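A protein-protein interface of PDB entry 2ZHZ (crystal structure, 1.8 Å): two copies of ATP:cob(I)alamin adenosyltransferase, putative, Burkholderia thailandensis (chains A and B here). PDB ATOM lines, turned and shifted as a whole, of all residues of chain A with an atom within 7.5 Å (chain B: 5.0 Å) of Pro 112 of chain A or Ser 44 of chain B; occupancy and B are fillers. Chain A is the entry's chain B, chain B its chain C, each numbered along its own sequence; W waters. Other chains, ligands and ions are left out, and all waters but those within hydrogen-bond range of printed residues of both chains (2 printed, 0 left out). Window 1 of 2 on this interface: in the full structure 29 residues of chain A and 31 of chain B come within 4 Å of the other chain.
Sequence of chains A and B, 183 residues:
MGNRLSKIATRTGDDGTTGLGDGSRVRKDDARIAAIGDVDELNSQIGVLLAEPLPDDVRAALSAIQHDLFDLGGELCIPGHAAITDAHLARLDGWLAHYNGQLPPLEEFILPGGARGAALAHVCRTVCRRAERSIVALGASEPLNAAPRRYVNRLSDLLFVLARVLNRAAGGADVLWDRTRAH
NE2 of Gln 66 of chain B is in hydrogen-bond range of O of Pro 112 of chain A (2.8 Å).
The side-chain hydroxyl of Ser 44 of chain B lies within hydrogen-bond range of the backbone carbonyl oxygen of His 122 of chain A (3.4 Å).
The guanidinium group (NH1) of Arg 125 of chain A lies within salt-bridge range of the side-chain carboxylate (OD1) of Asp 40 of chain B, 2.8 Å away.
The guanidinium group (NH2) of Arg 125 of chain A sits at hydrogen-bond distance from the side-chain hydroxyl (OG) of Ser 44 of chain B (3.4 Å).
Among the printed residues, pairs that only touch across the chains: Thr 126 of chain A with Ser 44 of chain B, Thr 126 of chain A with Glu 41 of chain B, Pro 112 of chain A with Ser 44 of chain B, Val 123 of chain A with Val 48 of chain B, Pro 112 of chain A with Gly 47 of chain B, Thr 126 of chain A with Asp 40 of chain B, Val 123 of chain A with Gln 45 of chain B, Ala 119 of chain A with Gly 47 of chain B, Pro 112 of chain A with Asn 43 of chain B, Val 123 of chain A with Ser 44 of chain B, Leu 111 of chain A with Gln 66 of chain B, Ala 119 of chain A with Val 48 of chain B and Val 127 of chain A with Glu 41 of chain B.
No position is printed for both chains.
The backbone NH (N) of Leu 111 of chain A sits at hydrogen-bond distance from the backbone carbonyl oxygen (O) of Val 175 of chain A, 2.6 Å away.
ND1 of His 122 of chain A is in hydrogen-bond range of NE of Arg 125 of chain A (3.0 Å).
OG1 of Thr 126 of chain A is in hydrogen-bond range of O of Val 123 of chain A, at 2.9 Å.
O of Asp 40 of chain B sits at hydrogen-bond distance from OG of Ser 44 of chain B (3.1 Å).
NE2 of Gln 66 of chain B lies within hydrogen-bond range of O of Asn 43 of chain B (3.1 Å).
Water W2 lies within hydrogen-bond range of the backbone carbonyl oxygen (O) of Ser 44 of chain B and the backbone carbonyl oxygen (O) of Ala 119 of chain A.
Water W1 lies within hydrogen-bond range of O of Gly 47 of chain B (2.7 Å) and N of Gly 114 of chain A (2.8 Å).
Printed residues of chain B that touch a printed residue of chain A: Asp 40, Glu 41, Asn 43, Ser 44, Gln 45, Gly 47, Val 48 and Gln 66.
Hydrophobic or aromatic side chains of chain B that line the printed part of chain A: Val 48.
Along chain B the printed residues that touch a printed residue of chain A span positions 40 to 66.
Hydrophobic or aromatic side chains of chain A that line the printed part of chain B: Leu 111, Pro 112, Ala 119, His 122, Val 123 and Val 127.
Among the printed residues, 17 pairs touch across the chains.
Ile 110 of chain A touches none of the printed residues of chain B.
Of chain B, only Asn 43, Ser 44, Gly 47 and Gln 66 come within 4 Å of Pro 112 of chain A.
Printed residues of chain B within 4 Å of Ala 119 of chain A: Gly 47 (3.6 Å) and Val 48 (3.8 Å).
Of the printed residues of chain B, Val 123 of chain A touches Ser 44 (3.7 Å), Gln 45 (3.6 Å) and Val 48 (3.5 Å).
Of the printed residues of chain B, Arg 125 of chain A touches Asp 40 and Ser 44.
Ser 44 of chain B touches just these residues of chain A: Pro 112 (3.4 Å), His 122 (3.4 Å), Val 123 (3.7 Å), Arg 125 (3.4 Å) and Thr 126 (3.2 Å).
The nearest residue of chain A that does not touch Ser 44 of chain B is Ala 119 of chain A (4.4 Å).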
ATOM      1  N   ILE A 110     -14.148 -21.448 -34.889  1.00  0.00           N
ATOM      2  CA  ILE A 110     -14.305 -20.331 -33.976  1.00  0.00           C
ATOM      3  C   ILE A 110     -13.632 -20.627 -32.646  1.00  0.00           C
ATOM      4  O   ILE A 110     -13.420 -21.784 -32.281  1.00  0.00           O
ATOM      5  CB  ILE A 110     -15.790 -19.989 -33.730  1.00  0.00           C
ATOM      6  CG1 ILE A 110     -16.480 -21.121 -32.978  1.00  0.00           C
ATOM      7  CG2 ILE A 110     -16.489 -19.737 -35.057  1.00  0.00           C
ATOM      8  CD1 ILE A 110     -17.922 -20.813 -32.639  1.00  0.00           C
ATOM      9  N   LEU A 111     -13.280 -19.563 -31.939  1.00  0.00           N
ATOM     10  CA  LEU A 111     -12.638 -19.675 -30.638  1.00  0.00           C
ATOM     11  C   LEU A 111     -13.706 -19.444 -29.577  1.00  0.00           C
ATOM     12  O   LEU A 111     -14.659 -18.694 -29.799  1.00  0.00           O
ATOM     13  CB  LEU A 111     -11.533 -18.623 -30.506  1.00  0.00           C
ATOM     14  CG  LEU A 111     -10.408 -18.702 -31.540  1.00  0.00           C
ATOM     15  CD1 LEU A 111      -9.424 -17.558 -31.332  1.00  0.00           C
ATOM     16  CD2 LEU A 111      -9.707 -20.044 -31.418  1.00  0.00           C
ATOM     17  N   PRO A 112     -13.566 -20.087 -28.409  1.00  0.00           N
ATOM     18  CA  PRO A 112     -14.567 -19.897 -27.354  1.00  0.00           C
ATOM     19  C   PRO A 112     -14.493 -18.499 -26.740  1.00  0.00           C
ATOM     20  O   PRO A 112     -13.462 -18.096 -26.206  1.00  0.00           O
ATOM     21  CB  PRO A 112     -14.235 -21.006 -26.358  1.00  0.00           C
ATOM     22  CG  PRO A 112     -12.737 -21.164 -26.517  1.00  0.00           C
ATOM     23  CD  PRO A 112     -12.545 -21.076 -28.013  1.00  0.00           C
ATOM     24  N   GLY A 113     -15.591 -17.756 -26.826  1.00  0.00           N
ATOM     25  CA  GLY A 113     -15.608 -16.413 -26.274  1.00  0.00           C
ATOM     26  C   GLY A 113     -16.611 -15.507 -26.956  1.00  0.00           C
ATOM     27  O   GLY A 113     -17.471 -15.975 -27.700  1.00  0.00           O
ATOM     28  N   GLY A 114     -16.492 -14.207 -26.707  1.00  0.00           N
ATOM     29  CA  GLY A 114     -17.408 -13.240 -27.292  1.00  0.00           C
ATOM     30  C   GLY A 114     -18.125 -12.504 -26.180  1.00  0.00           C
ATOM     31  O   GLY A 114     -17.487 -12.034 -25.241  1.00  0.00           O
ATOM     32  N   ALA A 118     -22.066 -15.774 -24.062  1.00  0.00           N
ATOM     33  CA  ALA A 118     -21.577 -16.763 -25.019  1.00  0.00           C
ATOM     34  C   ALA A 118     -20.314 -17.433 -24.487  1.00  0.00           C
ATOM     35  O   ALA A 118     -20.098 -18.631 -24.694  1.00  0.00           O
ATOM     36  CB  ALA A 118     -21.281 -16.098 -26.358  1.00  0.00           C
ATOM     37  N   ALA A 119     -19.474 -16.652 -23.813  1.00  0.00           N
ATOM     38  CA  ALA A 119     -18.237 -17.180 -23.246  1.00  0.00           C
ATOM     39  C   ALA A 119     -18.568 -18.201 -22.160  1.00  0.00           C
ATOM     40  O   ALA A 119     -17.947 -19.260 -22.077  1.00  0.00           O
ATOM     41  CB  ALA A 119     -17.399 -16.050 -22.663  1.00  0.00           C
ATOM     42  N   LEU A 120     -19.548 -17.877 -21.325  1.00  0.00           N
ATOM     43  CA  LEU A 120     -19.951 -18.783 -20.260  1.00  0.00           C
ATOM     44  C   LEU A 120     -20.552 -20.053 -20.858  1.00  0.00           C
ATOM     45  O   LEU A 120     -20.333 -21.151 -20.348  1.00  0.00           O
ATOM     46  CB  LEU A 120     -20.956 -18.096 -19.328  1.00  0.00           C
ATOM     47  CG  LEU A 120     -20.353 -17.015 -18.420  1.00  0.00           C
ATOM     48  CD1 LEU A 120     -21.463 -16.256 -17.693  1.00  0.00           C
ATOM     49  CD2 LEU A 120     -19.399 -17.670 -17.418  1.00  0.00           C
ATOM     50  N   ALA A 121     -21.296 -19.902 -21.951  1.00  0.00           N
ATOM     51  CA  ALA A 121     -21.904 -21.049 -22.609  1.00  0.00           C
ATOM     52  C   ALA A 121     -20.807 -22.001 -23.084  1.00  0.00           C
ATOM     53  O   ALA A 121     -20.976 -23.225 -23.054  1.00  0.00           O
ATOM     54  CB  ALA A 121     -22.758 -20.589 -23.794  1.00  0.00           C
ATOM     55  N   HIS A 122     -19.681 -21.440 -23.521  1.00  0.00           N
ATOM     56  CA  HIS A 122     -18.565 -22.264 -23.983  1.00  0.00           C
ATOM     57  C   HIS A 122     -17.914 -22.996 -22.813  1.00  0.00           C
ATOM     58  O   HIS A 122     -17.426 -24.112 -22.973  1.00  0.00           O
ATOM     59  CB  HIS A 122     -17.537 -21.410 -24.728  1.00  0.00           C
ATOM     60  CG  HIS A 122     -17.866 -21.210 -26.173  1.00  0.00           C
ATOM     61  ND1 HIS A 122     -17.814 -22.234 -27.095  1.00  0.00           N
ATOM     62  CD2 HIS A 122     -18.293 -20.117 -26.851  1.00  0.00           C
ATOM     63  CE1 HIS A 122     -18.198 -21.782 -28.276  1.00  0.00           C
ATOM     64  NE2 HIS A 122     -18.493 -20.500 -28.155  1.00  0.00           N
ATOM     65  N   VAL A 123     -17.900 -22.370 -21.641  1.00  0.00           N
ATOM     66  CA  VAL A 123     -17.349 -23.032 -20.463  1.00  0.00           C
ATOM     67  C   VAL A 123     -18.291 -24.199 -20.150  1.00  0.00           C
ATOM     68  O   VAL A 123     -17.843 -25.309 -19.862  1.00  0.00           O
ATOM     69  CB  VAL A 123     -17.269 -22.078 -19.248  1.00  0.00           C
ATOM     70  CG1 VAL A 123     -17.060 -22.881 -17.960  1.00  0.00           C
ATOM     71  CG2 VAL A 123     -16.106 -21.093 -19.440  1.00  0.00           C
ATOM     72  N   CYS A 124     -19.598 -23.951 -20.219  1.00  0.00           N
ATOM     73  CA  CYS A 124     -20.575 -25.007 -19.962  1.00  0.00           C
ATOM     74  C   CYS A 124     -20.346 -26.153 -20.945  1.00  0.00           C
ATOM     75  O   CYS A 124     -20.382 -27.325 -20.568  1.00  0.00           O
ATOM     76  CB  CYS A 124     -22.010 -24.479 -20.114  1.00  0.00           C
ATOM     77  SG  CYS A 124     -22.520 -23.325 -18.822  1.00  0.00           S
ATOM     78  N   ARG A 125     -20.107 -25.803 -22.205  1.00  0.00           N
ATOM     79  CA  ARG A 125     -19.860 -26.786 -23.252  1.00  0.00           C
ATOM     80  C   ARG A 125     -18.680 -27.692 -22.895  1.00  0.00           C
ATOM     81  O   ARG A 125     -18.785 -28.918 -22.980  1.00  0.00           O
ATOM     82  CB  ARG A 125     -19.591 -26.071 -24.585  1.00  0.00           C
ATOM     83  CG  ARG A 125     -19.165 -26.975 -25.743  1.00  0.00           C
ATOM     84  CD  ARG A 125     -18.830 -26.138 -26.973  1.00  0.00           C
ATOM     85  NE  ARG A 125     -17.709 -25.233 -26.713  1.00  0.00           N
ATOM     86  CZ  ARG A 125     -16.435 -25.609 -26.702  1.00  0.00           C
ATOM     87  NH1 ARG A 125     -16.111 -26.875 -26.945  1.00  0.00           N
ATOM     88  NH2 ARG A 125     -15.482 -24.726 -26.434  1.00  0.00           N
ATOM     89  N   THR A 126     -17.563 -27.096 -22.482  1.00  0.00           N
ATOM     90  CA  THR A 126     -16.390 -27.889 -22.133  1.00  0.00           C
ATOM     91  C   THR A 126     -16.577 -28.711 -20.858  1.00  0.00           C
ATOM     92  O   THR A 126     -16.054 -29.817 -20.758  1.00  0.00           O
ATOM     93  CB  THR A 126     -15.123 -27.012 -21.996  1.00  0.00           C
ATOM     94  OG1 THR A 126     -15.309 -26.043 -20.955  1.00  0.00           O
ATOM     95  CG2 THR A 126     -14.830 -26.306 -23.304  1.00  0.00           C
ATOM     96  N   VAL A 127     -17.309 -28.185 -19.880  1.00  0.00           N
ATOM     97  CA  VAL A 127     -17.532 -28.958 -18.665  1.00  0.00           C
ATOM     98  C   VAL A 127     -18.487 -30.103 -19.017  1.00  0.00           C
ATOM     99  O   VAL A 127     -18.393 -31.200 -18.462  1.00  0.00           O
ATOM    100  CB  VAL A 127     -18.133 -28.090 -17.537  1.00  0.00           C
ATOM    101  CG1 VAL A 127     -18.442 -28.958 -16.316  1.00  0.00           C
ATOM    102  CG2 VAL A 127     -17.142 -26.976 -17.157  1.00  0.00           C
ATOM    103  N   PHE A 160     -22.739 -25.231 -27.732  1.00  0.00           N
ATOM    104  CA  PHE A 160     -21.924 -24.562 -28.741  1.00  0.00           C
ATOM    105  C   PHE A 160     -22.859 -23.671 -29.565  1.00  0.00           C
ATOM    106  O   PHE A 160     -22.575 -22.501 -29.813  1.00  0.00           O
ATOM    107  CB  PHE A 160     -21.276 -25.597 -29.661  1.00  0.00           C
ATOM    108  CG  PHE A 160     -20.478 -25.002 -30.789  1.00  0.00           C
ATOM    109  CD1 PHE A 160     -19.166 -24.583 -30.591  1.00  0.00           C
ATOM    110  CD2 PHE A 160     -21.037 -24.876 -32.060  1.00  0.00           C
ATOM    111  CE1 PHE A 160     -18.414 -24.049 -31.644  1.00  0.00           C
ATOM    112  CE2 PHE A 160     -20.301 -24.346 -33.119  1.00  0.00           C
ATOM    113  CZ  PHE A 160     -18.984 -23.931 -32.912  1.00  0.00           C
ATOM    114  N   ALA A 163     -24.110 -20.669 -27.735  1.00  0.00           N
ATOM    115  CA  ALA A 163     -23.076 -19.648 -27.585  1.00  0.00           C
ATOM    116  C   ALA A 163     -23.145 -18.715 -28.802  1.00  0.00           C
ATOM    117  O   ALA A 163     -23.045 -17.497 -28.666  1.00  0.00           O
ATOM    118  CB  ALA A 163     -21.691 -20.297 -27.486  1.00  0.00           C
ATOM    119  N   ASN A 167     -24.058 -14.650 -28.931  1.00  0.00           N
ATOM    120  CA  ASN A 167     -23.208 -13.603 -29.483  1.00  0.00           C
ATOM    121  C   ASN A 167     -24.057 -12.715 -30.395  1.00  0.00           C
ATOM    122  O   ASN A 167     -23.904 -11.492 -30.407  1.00  0.00           O
ATOM    123  CB  ASN A 167     -22.028 -14.196 -30.261  1.00  0.00           C
ATOM    124  CG  ASN A 167     -20.807 -14.425 -29.379  1.00  0.00           C
ATOM    125  OD1 ASN A 167     -20.504 -13.610 -28.507  1.00  0.00           O
ATOM    126  ND2 ASN A 167     -20.092 -15.523 -29.616  1.00  0.00           N
ATOM    127  N   VAL A 175     -16.012 -15.345 -32.326  1.00  0.00           N
ATOM    128  CA  VAL A 175     -14.585 -15.070 -32.429  1.00  0.00           C
ATOM    129  C   VAL A 175     -13.999 -16.134 -33.347  1.00  0.00           C
ATOM    130  O   VAL A 175     -14.111 -17.327 -33.068  1.00  0.00           O
ATOM    131  CB  VAL A 175     -13.906 -15.156 -31.049  1.00  0.00           C
ATOM    132  CG1 VAL A 175     -12.443 -14.761 -31.162  1.00  0.00           C
ATOM    133  CG2 VAL A 175     -14.630 -14.258 -30.061  1.00  0.00           C
ATOM    134  N   LEU A 176     -13.377 -15.704 -34.441  1.00  0.00           N
ATOM    135  CA  LEU A 176     -12.816 -16.643 -35.402  1.00  0.00           C
ATOM    136  C   LEU A 176     -11.333 -16.956 -35.210  1.00  0.00           C
ATOM    137  O   LEU A 176     -10.550 -16.103 -34.792  1.00  0.00           O
ATOM    138  CB  LEU A 176     -13.041 -16.119 -36.823  1.00  0.00           C
ATOM    139  CG  LEU A 176     -14.483 -15.749 -37.179  1.00  0.00           C
ATOM    140  CD1 LEU A 176     -14.527 -15.180 -38.587  1.00  0.00           C
ATOM    141  CD2 LEU A 176     -15.380 -16.975 -37.066  1.00  0.00           C
ATOM    142  N   ASP B  40      -9.254 -27.319 -24.147  1.00  0.00           N
ATOM    143  CA  ASP B  40     -10.452 -26.630 -24.621  1.00  0.00           C
ATOM    144  C   ASP B  40     -11.115 -25.892 -23.450  1.00  0.00           C
ATOM    145  O   ASP B  40     -11.549 -24.745 -23.591  1.00  0.00           O
ATOM    146  CB  ASP B  40     -11.419 -27.659 -25.214  1.00  0.00           C
ATOM    147  CG  ASP B  40     -12.613 -27.025 -25.918  1.00  0.00           C
ATOM    148  OD1 ASP B  40     -13.562 -27.780 -26.226  1.00  0.00           O
ATOM    149  OD2 ASP B  40     -12.609 -25.797 -26.174  1.00  0.00           O
ATOM    150  N   GLU B  41     -11.187 -26.553 -22.294  1.00  0.00           N
ATOM    151  CA  GLU B  41     -11.802 -25.946 -21.116  1.00  0.00           C
ATOM    152  C   GLU B  41     -11.001 -24.716 -20.712  1.00  0.00           C
ATOM    153  O   GLU B  41     -11.566 -23.686 -20.363  1.00  0.00           O
ATOM    154  CB  GLU B  41     -11.861 -26.940 -19.950  1.00  0.00           C
ATOM    155  CG  GLU B  41     -12.721 -26.437 -18.789  1.00  0.00           C
ATOM    156  CD  GLU B  41     -12.938 -27.466 -17.689  1.00  0.00           C
ATOM    157  OE1 GLU B  41     -12.746 -28.679 -17.932  1.00  0.00           O
ATOM    158  OE2 GLU B  41     -13.319 -27.057 -16.573  1.00  0.00           O
ATOM    159  N   LEU B  42      -9.679 -24.832 -20.749  1.00  0.00           N
ATOM    160  CA  LEU B  42      -8.814 -23.703 -20.417  1.00  0.00           C
ATOM    161  C   LEU B  42      -9.077 -22.538 -21.373  1.00  0.00           C
ATOM    162  O   LEU B  42      -9.262 -21.397 -20.943  1.00  0.00           O
ATOM    163  CB  LEU B  42      -7.341 -24.108 -20.526  1.00  0.00           C
ATOM    164  CG  LEU B  42      -6.343 -22.945 -20.572  1.00  0.00           C
ATOM    165  CD1 LEU B  42      -6.385 -22.159 -19.261  1.00  0.00           C
ATOM    166  CD2 LEU B  42      -4.947 -23.491 -20.826  1.00  0.00           C
ATOM    167  N   ASN B  43      -9.079 -22.829 -22.669  1.00  0.00           N
ATOM    168  CA  ASN B  43      -9.312 -21.802 -23.681  1.00  0.00           C
ATOM    169  C   ASN B  43     -10.668 -21.133 -23.445  1.00  0.00           C
ATOM    170  O   ASN B  43     -10.819 -19.924 -23.657  1.00  0.00           O
ATOM    171  CB  ASN B  43      -9.252 -22.421 -25.082  1.00  0.00           C
ATOM    172  CG  ASN B  43      -8.882 -21.407 -26.157  1.00  0.00           C
ATOM    173  OD1 ASN B  43      -8.484 -20.280 -25.858  1.00  0.00           O
ATOM    174  ND2 ASN B  43      -9.001 -21.813 -27.420  1.00  0.00           N
ATOM    175  N   SER B  44     -11.651 -21.913 -23.000  1.00  0.00           N
ATOM    176  CA  SER B  44     -12.975 -21.362 -22.726  1.00  0.00           C
ATOM    177  C   SER B  44     -12.947 -20.431 -21.518  1.00  0.00           C
ATOM    178  O   SER B  44     -13.604 -19.385 -21.521  1.00  0.00           O
ATOM    179  CB  SER B  44     -13.990 -22.487 -22.510  1.00  0.00           C
ATOM    180  OG  SER B  44     -14.204 -23.178 -23.736  1.00  0.00           O
ATOM    181  N   GLN B  45     -12.190 -20.801 -20.486  1.00  0.00           N
ATOM    182  CA  GLN B  45     -12.083 -19.951 -19.301  1.00  0.00           C
ATOM    183  C   GLN B  45     -11.387 -18.643 -19.676  1.00  0.00           C
ATOM    184  O   GLN B  45     -11.708 -17.581 -19.139  1.00  0.00           O
ATOM    185  CB  GLN B  45     -11.307 -20.663 -18.185  1.00  0.00           C
ATOM    186  CG  GLN B  45     -12.128 -21.687 -17.406  1.00  0.00           C
ATOM    187  CD  GLN B  45     -13.261 -21.049 -16.600  1.00  0.00           C
ATOM    188  OE1 GLN B  45     -13.314 -19.829 -16.437  1.00  0.00           O
ATOM    189  NE2 GLN B  45     -14.164 -21.877 -16.084  1.00  0.00           N
ATOM    190  N   ILE B  46     -10.437 -18.717 -20.603  1.00  0.00           N
ATOM    191  CA  ILE B  46      -9.741 -17.518 -21.049  1.00  0.00           C
ATOM    192  C   ILE B  46     -10.752 -16.649 -21.806  1.00  0.00           C
ATOM    193  O   ILE B  46     -10.682 -15.423 -21.770  1.00  0.00           O
ATOM    194  CB  ILE B  46      -8.531 -17.878 -21.949  1.00  0.00           C
ATOM    195  CG1 ILE B  46      -7.425 -18.479 -21.077  1.00  0.00           C
ATOM    196  CG2 ILE B  46      -8.029 -16.633 -22.702  1.00  0.00           C
ATOM    197  CD1 ILE B  46      -6.191 -18.939 -21.832  1.00  0.00           C
ATOM    198  N   GLY B  47     -11.703 -17.299 -22.473  1.00  0.00           N
ATOM    199  CA  GLY B  47     -12.734 -16.570 -23.195  1.00  0.00           C
ATOM    200  C   GLY B  47     -13.591 -15.757 -22.236  1.00  0.00           C
ATOM    201  O   GLY B  47     -14.045 -14.656 -22.568  1.00  0.00           O
ATOM    202  N   VAL B  48     -13.822 -16.297 -21.042  1.00  0.00           N
ATOM    203  CA  VAL B  48     -14.612 -15.595 -20.034  1.00  0.00           C
ATOM    204  C   VAL B  48     -13.814 -14.400 -19.516  1.00  0.00           C
ATOM    205  O   VAL B  48     -14.366 -13.321 -19.290  1.00  0.00           O
ATOM    206  CB  VAL B  48     -14.969 -16.529 -18.848  1.00  0.00           C
ATOM    207  CG1 VAL B  48     -15.653 -15.735 -17.733  1.00  0.00           C
ATOM    208  CG2 VAL B  48     -15.883 -17.649 -19.335  1.00  0.00           C
ATOM    209  N   GLN B  66      -5.376 -17.614 -27.230  1.00  0.00           N
ATOM    210  CA  GLN B  66      -6.529 -18.418 -27.622  1.00  0.00           C
ATOM    211  C   GLN B  66      -6.276 -19.119 -28.956  1.00  0.00           C
ATOM    212  O   GLN B  66      -6.732 -20.245 -29.170  1.00  0.00           O
ATOM    213  CB  GLN B  66      -7.790 -17.556 -27.736  1.00  0.00           C
ATOM    214  CG  GLN B  66      -8.434 -17.213 -26.405  1.00  0.00           C
ATOM    215  CD  GLN B  66      -9.921 -16.966 -26.553  1.00  0.00           C
ATOM    216  OE1 GLN B  66     -10.341 -16.065 -27.282  1.00  0.00           O
ATOM    217  NE2 GLN B  66     -10.728 -17.777 -25.873  1.00  0.00           N
HETATM  218  O   HOH W   1     -14.348 -13.565 -25.053  1.00  0.00           O
HETATM  219  O   HOH W   2     -15.480 -18.924 -23.431  1.00  0.00           O
